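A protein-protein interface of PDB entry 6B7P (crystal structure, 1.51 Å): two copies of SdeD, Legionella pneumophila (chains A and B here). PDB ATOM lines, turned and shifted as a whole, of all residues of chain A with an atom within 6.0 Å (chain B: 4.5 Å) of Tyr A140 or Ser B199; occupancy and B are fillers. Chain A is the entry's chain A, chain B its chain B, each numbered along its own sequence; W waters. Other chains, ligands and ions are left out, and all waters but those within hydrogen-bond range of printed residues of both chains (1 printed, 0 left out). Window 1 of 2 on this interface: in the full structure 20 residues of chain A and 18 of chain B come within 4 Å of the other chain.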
ATOM      1  N   GLU A  28     -17.033 -24.095 -17.300  1.00  0.00           N
ATOM      2  CA  GLU A  28     -17.169 -23.449 -16.049  1.00  0.00           C
ATOM      3  C   GLU A  28     -17.690 -22.021 -16.358  1.00  0.00           C
ATOM      4  O   GLU A  28     -17.052 -21.011 -16.155  1.00  0.00           O
ATOM      5  CB  GLU A  28     -15.864 -23.404 -15.244  1.00  0.00           C
ATOM      6  CG  GLU A  28     -15.336 -24.718 -14.765  1.00  0.00           C
ATOM      7  CD  GLU A  28     -14.056 -24.553 -13.904  1.00  0.00           C
ATOM      8  OE1 GLU A  28     -13.597 -23.459 -13.612  1.00  0.00           O
ATOM      9  OE2 GLU A  28     -13.585 -25.640 -13.500  1.00  0.00           O
ATOM     10  N   ALA A 122      -5.144 -26.121 -23.225  1.00  0.00           N
ATOM     11  CA  ALA A 122      -6.195 -27.010 -23.638  1.00  0.00           C
ATOM     12  C   ALA A 122      -7.141 -27.416 -22.501  1.00  0.00           C
ATOM     13  O   ALA A 122      -8.234 -27.730 -22.727  1.00  0.00           O
ATOM     14  CB  ALA A 122      -5.596 -28.234 -24.327  1.00  0.00           C
ATOM     15  N   GLY A 123      -6.637 -27.354 -21.290  1.00  0.00           N
ATOM     16  CA  GLY A 123      -7.425 -27.689 -20.129  1.00  0.00           C
ATOM     17  C   GLY A 123      -8.316 -26.579 -19.560  1.00  0.00           C
ATOM     18  O   GLY A 123      -9.039 -26.808 -18.681  1.00  0.00           O
ATOM     19  N   ARG A 124      -8.224 -25.381 -20.125  1.00  0.00           N
ATOM     20  CA  ARG A 124      -9.035 -24.258 -19.666  1.00  0.00           C
ATOM     21  C   ARG A 124     -10.528 -24.537 -19.827  1.00  0.00           C
ATOM     22  O   ARG A 124     -10.953 -25.130 -20.819  1.00  0.00           O
ATOM     23  CB  ARG A 124      -8.655 -22.980 -20.417  1.00  0.00           C
ATOM     24  CG  ARG A 124      -7.246 -22.488 -20.132  1.00  0.00           C
ATOM     25  CD  ARG A 124      -7.078 -21.030 -20.531  1.00  0.00           C
ATOM     26  NE  ARG A 124      -8.002 -20.157 -19.811  1.00  0.00           N
ATOM     27  CZ  ARG A 124      -7.691 -19.495 -18.701  1.00  0.00           C
ATOM     28  NH1 ARG A 124      -6.478 -19.604 -18.179  1.00  0.00           N
ATOM     29  NH2 ARG A 124      -8.595 -18.722 -18.114  1.00  0.00           N
ATOM     30  N   GLU A 125     -11.317 -24.107 -18.848  1.00  0.00           N
ATOM     31  CA  GLU A 125     -12.748 -24.293 -18.886  1.00  0.00           C
ATOM     32  C   GLU A 125     -13.502 -22.978 -18.787  1.00  0.00           C
ATOM     33  O   GLU A 125     -14.685 -22.990 -18.695  1.00  0.00           O
ATOM     34  CB  GLU A 125     -13.192 -25.252 -17.794  1.00  0.00           C
ATOM     35  CG  GLU A 125     -12.780 -26.706 -18.026  1.00  0.00           C
ATOM     36  CD  GLU A 125     -13.317 -27.303 -19.338  1.00  0.00           C
ATOM     37  OE1 GLU A 125     -14.281 -26.795 -19.887  1.00  0.00           O
ATOM     38  OE2 GLU A 125     -12.777 -28.280 -19.793  1.00  0.00           O
ATOM     39  N   HIS A 135      -4.568 -22.659 -12.131  1.00  0.00           N
ATOM     40  CA  HIS A 135      -3.856 -23.859 -11.742  1.00  0.00           C
ATOM     41  C   HIS A 135      -4.660 -25.135 -11.997  1.00  0.00           C
ATOM     42  O   HIS A 135      -4.139 -26.184 -12.453  1.00  0.00           O
ATOM     43  CB  HIS A 135      -3.327 -23.781 -10.315  1.00  0.00           C
ATOM     44  CG  HIS A 135      -2.145 -22.927 -10.185  1.00  0.00           C
ATOM     45  ND1 HIS A 135      -0.921 -23.227 -10.791  1.00  0.00           N
ATOM     46  CD2 HIS A 135      -2.000 -21.652  -9.725  1.00  0.00           C
ATOM     47  CE1 HIS A 135      -0.075 -22.220 -10.595  1.00  0.00           C
ATOM     48  NE2 HIS A 135      -0.708 -21.249  -9.949  1.00  0.00           N
ATOM     49  N   ARG A 136      -5.977 -25.124 -11.745  1.00  0.00           N
ATOM     50  CA  ARG A 136      -6.829 -26.238 -12.107  1.00  0.00           C
ATOM     51  C   ARG A 136      -6.791 -26.484 -13.612  1.00  0.00           C
ATOM     52  O   ARG A 136      -6.693 -27.636 -14.043  1.00  0.00           O
ATOM     53  CB  ARG A 136      -8.268 -25.938 -11.615  1.00  0.00           C
ATOM     54  CG  ARG A 136      -9.258 -26.987 -12.059  1.00  0.00           C
ATOM     55  CD  ARG A 136     -10.635 -26.930 -11.352  1.00  0.00           C
ATOM     56  NE  ARG A 136     -11.349 -25.699 -11.637  1.00  0.00           N
ATOM     57  CZ  ARG A 136     -11.406 -24.642 -10.823  1.00  0.00           C
ATOM     58  NH1 ARG A 136     -12.087 -23.599 -11.198  1.00  0.00           N
ATOM     59  NH2 ARG A 136     -10.758 -24.628  -9.661  1.00  0.00           N
ATOM     60  N   TYR A 137      -6.898 -25.440 -14.404  1.00  0.00           N
ATOM     61  CA  TYR A 137      -6.904 -25.563 -15.865  1.00  0.00           C
ATOM     62  C   TYR A 137      -5.585 -26.131 -16.414  1.00  0.00           C
ATOM     63  O   TYR A 137      -5.563 -26.873 -17.341  1.00  0.00           O
ATOM     64  CB  TYR A 137      -7.219 -24.228 -16.542  1.00  0.00           C
ATOM     65  CG  TYR A 137      -8.596 -23.655 -16.206  1.00  0.00           C
ATOM     66  CD1 TYR A 137      -9.551 -24.413 -15.638  1.00  0.00           C
ATOM     67  CD2 TYR A 137      -8.879 -22.341 -16.432  1.00  0.00           C
ATOM     68  CE1 TYR A 137     -10.761 -23.864 -15.322  1.00  0.00           C
ATOM     69  CE2 TYR A 137     -10.091 -21.795 -16.114  1.00  0.00           C
ATOM     70  CZ  TYR A 137     -11.023 -22.550 -15.557  1.00  0.00           C
ATOM     71  OH  TYR A 137     -12.228 -21.956 -15.262  1.00  0.00           O
ATOM     72  N   HIS A 138      -4.494 -25.732 -15.801  1.00  0.00           N
ATOM     73  CA  HIS A 138      -3.150 -26.257 -16.229  1.00  0.00           C
ATOM     74  C   HIS A 138      -2.974 -27.706 -15.771  1.00  0.00           C
ATOM     75  O   HIS A 138      -2.438 -28.489 -16.539  1.00  0.00           O
ATOM     76  CB  HIS A 138      -2.072 -25.314 -15.795  1.00  0.00           C
ATOM     77  CG  HIS A 138      -1.910 -24.208 -16.765  1.00  0.00           C
ATOM     78  ND1 HIS A 138      -1.016 -24.264 -17.856  1.00  0.00           N
ATOM     79  CD2 HIS A 138      -2.643 -23.096 -16.982  1.00  0.00           C
ATOM     80  CE1 HIS A 138      -1.167 -23.226 -18.636  1.00  0.00           C
ATOM     81  NE2 HIS A 138      -2.151 -22.491 -18.161  1.00  0.00           N
ATOM     82  N   LEU A 139      -3.506 -28.112 -14.613  1.00  0.00           N
ATOM     83  CA  LEU A 139      -3.493 -29.477 -14.205  1.00  0.00           C
ATOM     84  C   LEU A 139      -4.338 -30.272 -15.178  1.00  0.00           C
ATOM     85  O   LEU A 139      -3.903 -31.337 -15.708  1.00  0.00           O
ATOM     86  CB  LEU A 139      -4.035 -29.599 -12.818  1.00  0.00           C
ATOM     87  CG  LEU A 139      -4.079 -31.031 -12.306  1.00  0.00           C
ATOM     88  CD1 LEU A 139      -2.757 -31.629 -12.285  1.00  0.00           C
ATOM     89  CD2 LEU A 139      -4.422 -31.027 -10.806  1.00  0.00           C
ATOM     90  N   TYR A 140      -5.506 -29.793 -15.533  1.00  0.00           N
ATOM     91  CA  TYR A 140      -6.301 -30.511 -16.487  1.00  0.00           C
ATOM     92  C   TYR A 140      -5.600 -30.687 -17.845  1.00  0.00           C
ATOM     93  O   TYR A 140      -5.693 -31.722 -18.401  1.00  0.00           O
ATOM     94  CB  TYR A 140      -7.577 -29.765 -16.761  1.00  0.00           C
ATOM     95  CG  TYR A 140      -8.672 -29.816 -15.719  1.00  0.00           C
ATOM     96  CD1 TYR A 140      -8.751 -30.778 -14.766  1.00  0.00           C
ATOM     97  CD2 TYR A 140      -9.645 -28.884 -15.774  1.00  0.00           C
ATOM     98  CE1 TYR A 140      -9.816 -30.790 -13.878  1.00  0.00           C
ATOM     99  CE2 TYR A 140     -10.684 -28.889 -14.905  1.00  0.00           C
ATOM    100  CZ  TYR A 140     -10.757 -29.834 -13.967  1.00  0.00           C
ATOM    101  OH  TYR A 140     -11.846 -29.808 -13.135  1.00  0.00           O
ATOM    102  N   GLY A 141      -4.944 -29.655 -18.364  1.00  0.00           N
ATOM    103  CA  GLY A 141      -4.260 -29.778 -19.671  1.00  0.00           C
ATOM    104  C   GLY A 141      -3.100 -30.745 -19.541  1.00  0.00           C
ATOM    105  O   GLY A 141      -2.790 -31.422 -20.536  1.00  0.00           O
ATOM    106  N   ALA A 142      -2.376 -30.713 -18.460  1.00  0.00           N
ATOM    107  CA  ALA A 142      -1.219 -31.636 -18.247  1.00  0.00           C
ATOM    108  C   ALA A 142      -1.715 -33.069 -18.281  1.00  0.00           C
ATOM    109  O   ALA A 142      -1.072 -33.948 -18.914  1.00  0.00           O
ATOM    110  CB  ALA A 142      -0.570 -31.329 -16.923  1.00  0.00           C
ATOM    111  N   LYS A 143      -2.878 -33.362 -17.698  1.00  0.00           N
ATOM    112  CA  LYS A 143      -3.403 -34.721 -17.699  1.00  0.00           C
ATOM    113  C   LYS A 143      -4.003 -35.084 -19.025  1.00  0.00           C
ATOM    114  O   LYS A 143      -3.859 -36.275 -19.472  1.00  0.00           O
ATOM    115  CB  LYS A 143      -4.418 -34.931 -16.622  1.00  0.00           C
ATOM    116  CG  LYS A 143      -3.872 -34.678 -15.241  1.00  0.00           C
ATOM    117  CD  LYS A 143      -2.756 -35.602 -14.843  1.00  0.00           C
ATOM    118  CE  LYS A 143      -2.926 -35.910 -13.343  1.00  0.00           C
ATOM    119  NZ  LYS A 143      -4.106 -36.833 -13.162  1.00  0.00           N
ATOM    120  N   GLN A 144      -4.546 -34.160 -19.761  1.00  0.00           N
ATOM    121  CA  GLN A 144      -4.984 -34.396 -21.145  1.00  0.00           C
ATOM    122  C   GLN A 144      -3.795 -34.716 -22.037  1.00  0.00           C
ATOM    123  O   GLN A 144      -3.843 -35.705 -22.847  1.00  0.00           O
ATOM    124  CB  GLN A 144      -5.767 -33.250 -21.726  1.00  0.00           C
ATOM    125  CG  GLN A 144      -7.132 -33.094 -21.098  1.00  0.00           C
ATOM    126  CD  GLN A 144      -7.720 -31.682 -21.088  1.00  0.00           C
ATOM    127  OE1 GLN A 144      -7.247 -30.731 -21.700  1.00  0.00           O
ATOM    128  NE2 GLN A 144      -8.848 -31.574 -20.382  1.00  0.00           N
ATOM    129  N   PHE A 145      -2.662 -34.030 -21.865  1.00  0.00           N
ATOM    130  CA  PHE A 145      -1.453 -34.397 -22.573  1.00  0.00           C
ATOM    131  C   PHE A 145      -0.951 -35.773 -22.126  1.00  0.00           C
ATOM    132  O   PHE A 145      -0.605 -36.561 -23.078  1.00  0.00           O
ATOM    133  CB  PHE A 145      -0.350 -33.382 -22.217  1.00  0.00           C
ATOM    134  CG  PHE A 145       1.033 -33.777 -22.699  1.00  0.00           C
ATOM    135  CD1 PHE A 145       1.366 -33.790 -24.027  1.00  0.00           C
ATOM    136  CD2 PHE A 145       1.893 -34.279 -21.788  1.00  0.00           C
ATOM    137  CE1 PHE A 145       2.623 -34.229 -24.429  1.00  0.00           C
ATOM    138  CE2 PHE A 145       3.156 -34.750 -22.193  1.00  0.00           C
ATOM    139  CZ  PHE A 145       3.505 -34.714 -23.515  1.00  0.00           C
ATOM    140  N   CYS B 197     -19.791 -36.403 -18.222  1.00  0.00           N
ATOM    141  CA  CYS B 197     -19.524 -35.029 -18.758  1.00  0.00           C
ATOM    142  C   CYS B 197     -19.115 -34.045 -17.680  1.00  0.00           C
ATOM    143  O   CYS B 197     -18.665 -32.910 -17.977  1.00  0.00           O
ATOM    144  CB  CYS B 197     -20.712 -34.439 -19.505  1.00  0.00           C
ATOM    145  SG  CYS B 197     -22.325 -34.717 -18.743  1.00  0.00           S
ATOM    146  N   LYS B 198     -19.191 -34.442 -16.430  1.00  0.00           N
ATOM    147  CA  LYS B 198     -18.925 -33.523 -15.351  1.00  0.00           C
ATOM    148  C   LYS B 198     -17.535 -33.645 -14.806  1.00  0.00           C
ATOM    149  O   LYS B 198     -16.887 -34.608 -15.022  1.00  0.00           O
ATOM    150  CB  LYS B 198     -19.945 -33.676 -14.226  1.00  0.00           C
ATOM    151  CG  LYS B 198     -21.338 -33.377 -14.686  1.00  0.00           C
ATOM    152  CD  LYS B 198     -21.559 -31.903 -14.696  1.00  0.00           C
ATOM    153  CE  LYS B 198     -21.800 -31.437 -16.087  1.00  0.00           C
ATOM    154  NZ  LYS B 198     -23.232 -31.262 -16.386  1.00  0.00           N
ATOM    155  N   SER B 199     -17.063 -32.619 -14.102  1.00  0.00           N
ATOM    156  CA  SER B 199     -15.671 -32.580 -13.638  1.00  0.00           C
ATOM    157  C   SER B 199     -15.406 -33.438 -12.399  1.00  0.00           C
ATOM    158  O   SER B 199     -16.342 -33.912 -11.755  1.00  0.00           O
ATOM    159  CB  SER B 199     -15.239 -31.135 -13.375  1.00  0.00           C
ATOM    160  OG  SER B 199     -15.786 -30.654 -12.159  1.00  0.00           O
ATOM    161  N   PRO B 200     -14.129 -33.634 -12.064  1.00  0.00           N
ATOM    162  CA  PRO B 200     -13.774 -34.416 -10.874  1.00  0.00           C
ATOM    163  C   PRO B 200     -14.382 -33.825  -9.601  1.00  0.00           C
ATOM    164  O   PRO B 200     -14.680 -34.552  -8.654  1.00  0.00           O
ATOM    165  CB  PRO B 200     -12.249 -34.304 -10.829  1.00  0.00           C
ATOM    166  CG  PRO B 200     -11.851 -34.106 -12.252  1.00  0.00           C
ATOM    167  CD  PRO B 200     -12.947 -33.289 -12.875  1.00  0.00           C
ATOM    168  N   VAL B 201     -14.559 -32.509  -9.599  1.00  0.00           N
ATOM    169  CA  VAL B 201     -15.114 -31.788  -8.486  1.00  0.00           C
ATOM    170  C   VAL B 201     -16.570 -32.220  -8.284  1.00  0.00           C
ATOM    171  O   VAL B 201     -16.942 -32.592  -7.233  1.00  0.00           O
ATOM    172  CB  VAL B 201     -15.009 -30.253  -8.656  1.00  0.00           C
ATOM    173  CG1 VAL B 201     -15.787 -29.561  -7.576  1.00  0.00           C
ATOM    174  CG2 VAL B 201     -13.563 -29.788  -8.655  1.00  0.00           C
ATOM    175  N   GLU B 202     -17.357 -32.167  -9.345  1.00  0.00           N
ATOM    176  CA  GLU B 202     -18.741 -32.550  -9.263  1.00  0.00           C
ATOM    177  C   GLU B 202     -18.924 -34.039  -8.986  1.00  0.00           C
ATOM    178  O   GLU B 202     -19.776 -34.435  -8.253  1.00  0.00           O
ATOM    179  CB  GLU B 202     -19.470 -32.122 -10.531  1.00  0.00           C
ATOM    180  CG  GLU B 202     -20.891 -32.588 -10.639  1.00  0.00           C
ATOM    181  CD  GLU B 202     -21.773 -31.646 -11.448  1.00  0.00           C
ATOM    182  OE1 GLU B 202     -22.999 -31.875 -11.465  1.00  0.00           O
ATOM    183  OE2 GLU B 202     -21.232 -30.688 -12.047  1.00  0.00           O
ATOM    184  N   VAL B 203     -18.079 -34.846  -9.570  1.00  0.00           N
ATOM    185  CA  VAL B 203     -18.233 -36.330  -9.418  1.00  0.00           C
ATOM    186  C   VAL B 203     -17.783 -36.836  -8.007  1.00  0.00           C
ATOM    187  O   VAL B 203     -18.352 -37.821  -7.473  1.00  0.00           O
ATOM    188  CB  VAL B 203     -17.527 -37.054 -10.554  1.00  0.00           C
ATOM    189  CG1 VAL B 203     -17.634 -38.562 -10.419  1.00  0.00           C
ATOM    190  CG2 VAL B 203     -18.152 -36.696 -11.896  1.00  0.00           C
ATOM    191  N   TYR B 247     -10.952 -40.311 -17.265  1.00  0.00           N
ATOM    192  CA  TYR B 247     -10.066 -40.921 -16.324  1.00  0.00           C
ATOM    193  C   TYR B 247     -10.454 -40.506 -14.897  1.00  0.00           C
ATOM    194  O   TYR B 247     -11.164 -39.470 -14.719  1.00  0.00           O
ATOM    195  CB  TYR B 247      -8.582 -40.463 -16.625  1.00  0.00           C
ATOM    196  CG  TYR B 247      -8.316 -39.016 -16.282  1.00  0.00           C
ATOM    197  CD1 TYR B 247      -8.130 -38.589 -14.953  1.00  0.00           C
ATOM    198  CD2 TYR B 247      -8.230 -38.053 -17.271  1.00  0.00           C
ATOM    199  CE1 TYR B 247      -7.914 -37.257 -14.630  1.00  0.00           C
ATOM    200  CE2 TYR B 247      -7.978 -36.674 -16.975  1.00  0.00           C
ATOM    201  CZ  TYR B 247      -7.797 -36.281 -15.645  1.00  0.00           C
ATOM    202  OH  TYR B 247      -7.627 -34.895 -15.298  1.00  0.00           O
ATOM    203  N   LEU B 256      -7.336 -29.116  -6.958  1.00  0.00           N
ATOM    204  CA  LEU B 256      -8.378 -28.580  -7.807  1.00  0.00           C
ATOM    205  C   LEU B 256      -9.041 -27.317  -7.262  1.00  0.00           C
ATOM    206  O   LEU B 256      -9.921 -26.818  -7.889  1.00  0.00           O
ATOM    207  CB  LEU B 256      -9.426 -29.656  -8.113  1.00  0.00           C
ATOM    208  CG  LEU B 256      -8.998 -30.951  -8.786  1.00  0.00           C
ATOM    209  CD1 LEU B 256     -10.138 -31.938  -8.783  1.00  0.00           C
ATOM    210  CD2 LEU B 256      -8.516 -30.774 -10.200  1.00  0.00           C
HETATM  211  O   HOH W   1      -7.868 -33.440 -17.495  1.00  0.00           O
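The guanidinium group (NH2) of Arg A136 lies within hydrogen-bond range of the backbone carbonyl oxygen (O) of Leu B256 (2.9 Å).
The guanidinium group (NH1) of Arg A136 lies within salt-bridge range of the side-chain carboxylate (OE1) of Glu A28, at 2.9 Å. The side-chain hydroxyl (OG) of Ser B199 sits close to the backbone NH (N) of Val B201 (3.4 Å).
Among the printed residues, merely in contact across the chains: Lys A143 with Tyr B247 (3.5 Å), Tyr A140 with Ser B199 (3.7 Å), Tyr A140 with Pro B200 (3.7 Å) and Tyr A140 with Leu B256 (3.9 Å).
Tyr A140 touches just these residues of chain B: Ser B199, Pro B200 and Leu B256. Ser B199 touches just one residue of chain A: Tyr A140. Printed residues of chain A within 4 Å of Tyr B247: Lys A143 (3.5 Å). Printed residues of chain A within 4 Å of Pro B200: Tyr A140 (3.7 Å). Printed residues of chain B within 4 Å of Lys A143: Tyr B247. The nearest residue of chain B that does not touch Tyr A140 is Tyr B247 (4.3 Å). The nearest residue of chain A that does not touch Ser B199 is Glu A28 (5.6 Å). The nearest printed residue of chain B that does not touch Arg A136 is Val B201 (4.9 Å).
Of the 9 printed residues of chain B, 4 touch a printed residue of chain A. Hydrophobic or aromatic side chains of chain B within 4 Å of the printed part of chain A: Pro B200, Tyr B247 and Leu B256. Along chain A the printed residues that touch a printed residue of chain B span positions 136 to 143. Among the printed residues, 5 pairs touch across the chains. Among the printed residues, no Asp or Glu carboxylate lies within 4 Å of a Lys or Arg side-chain nitrogen of the other chain.
No position is printed for both chains.
Water W1 lies within hydrogen-bond range of OH of Tyr B247 and O of Tyr A140.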
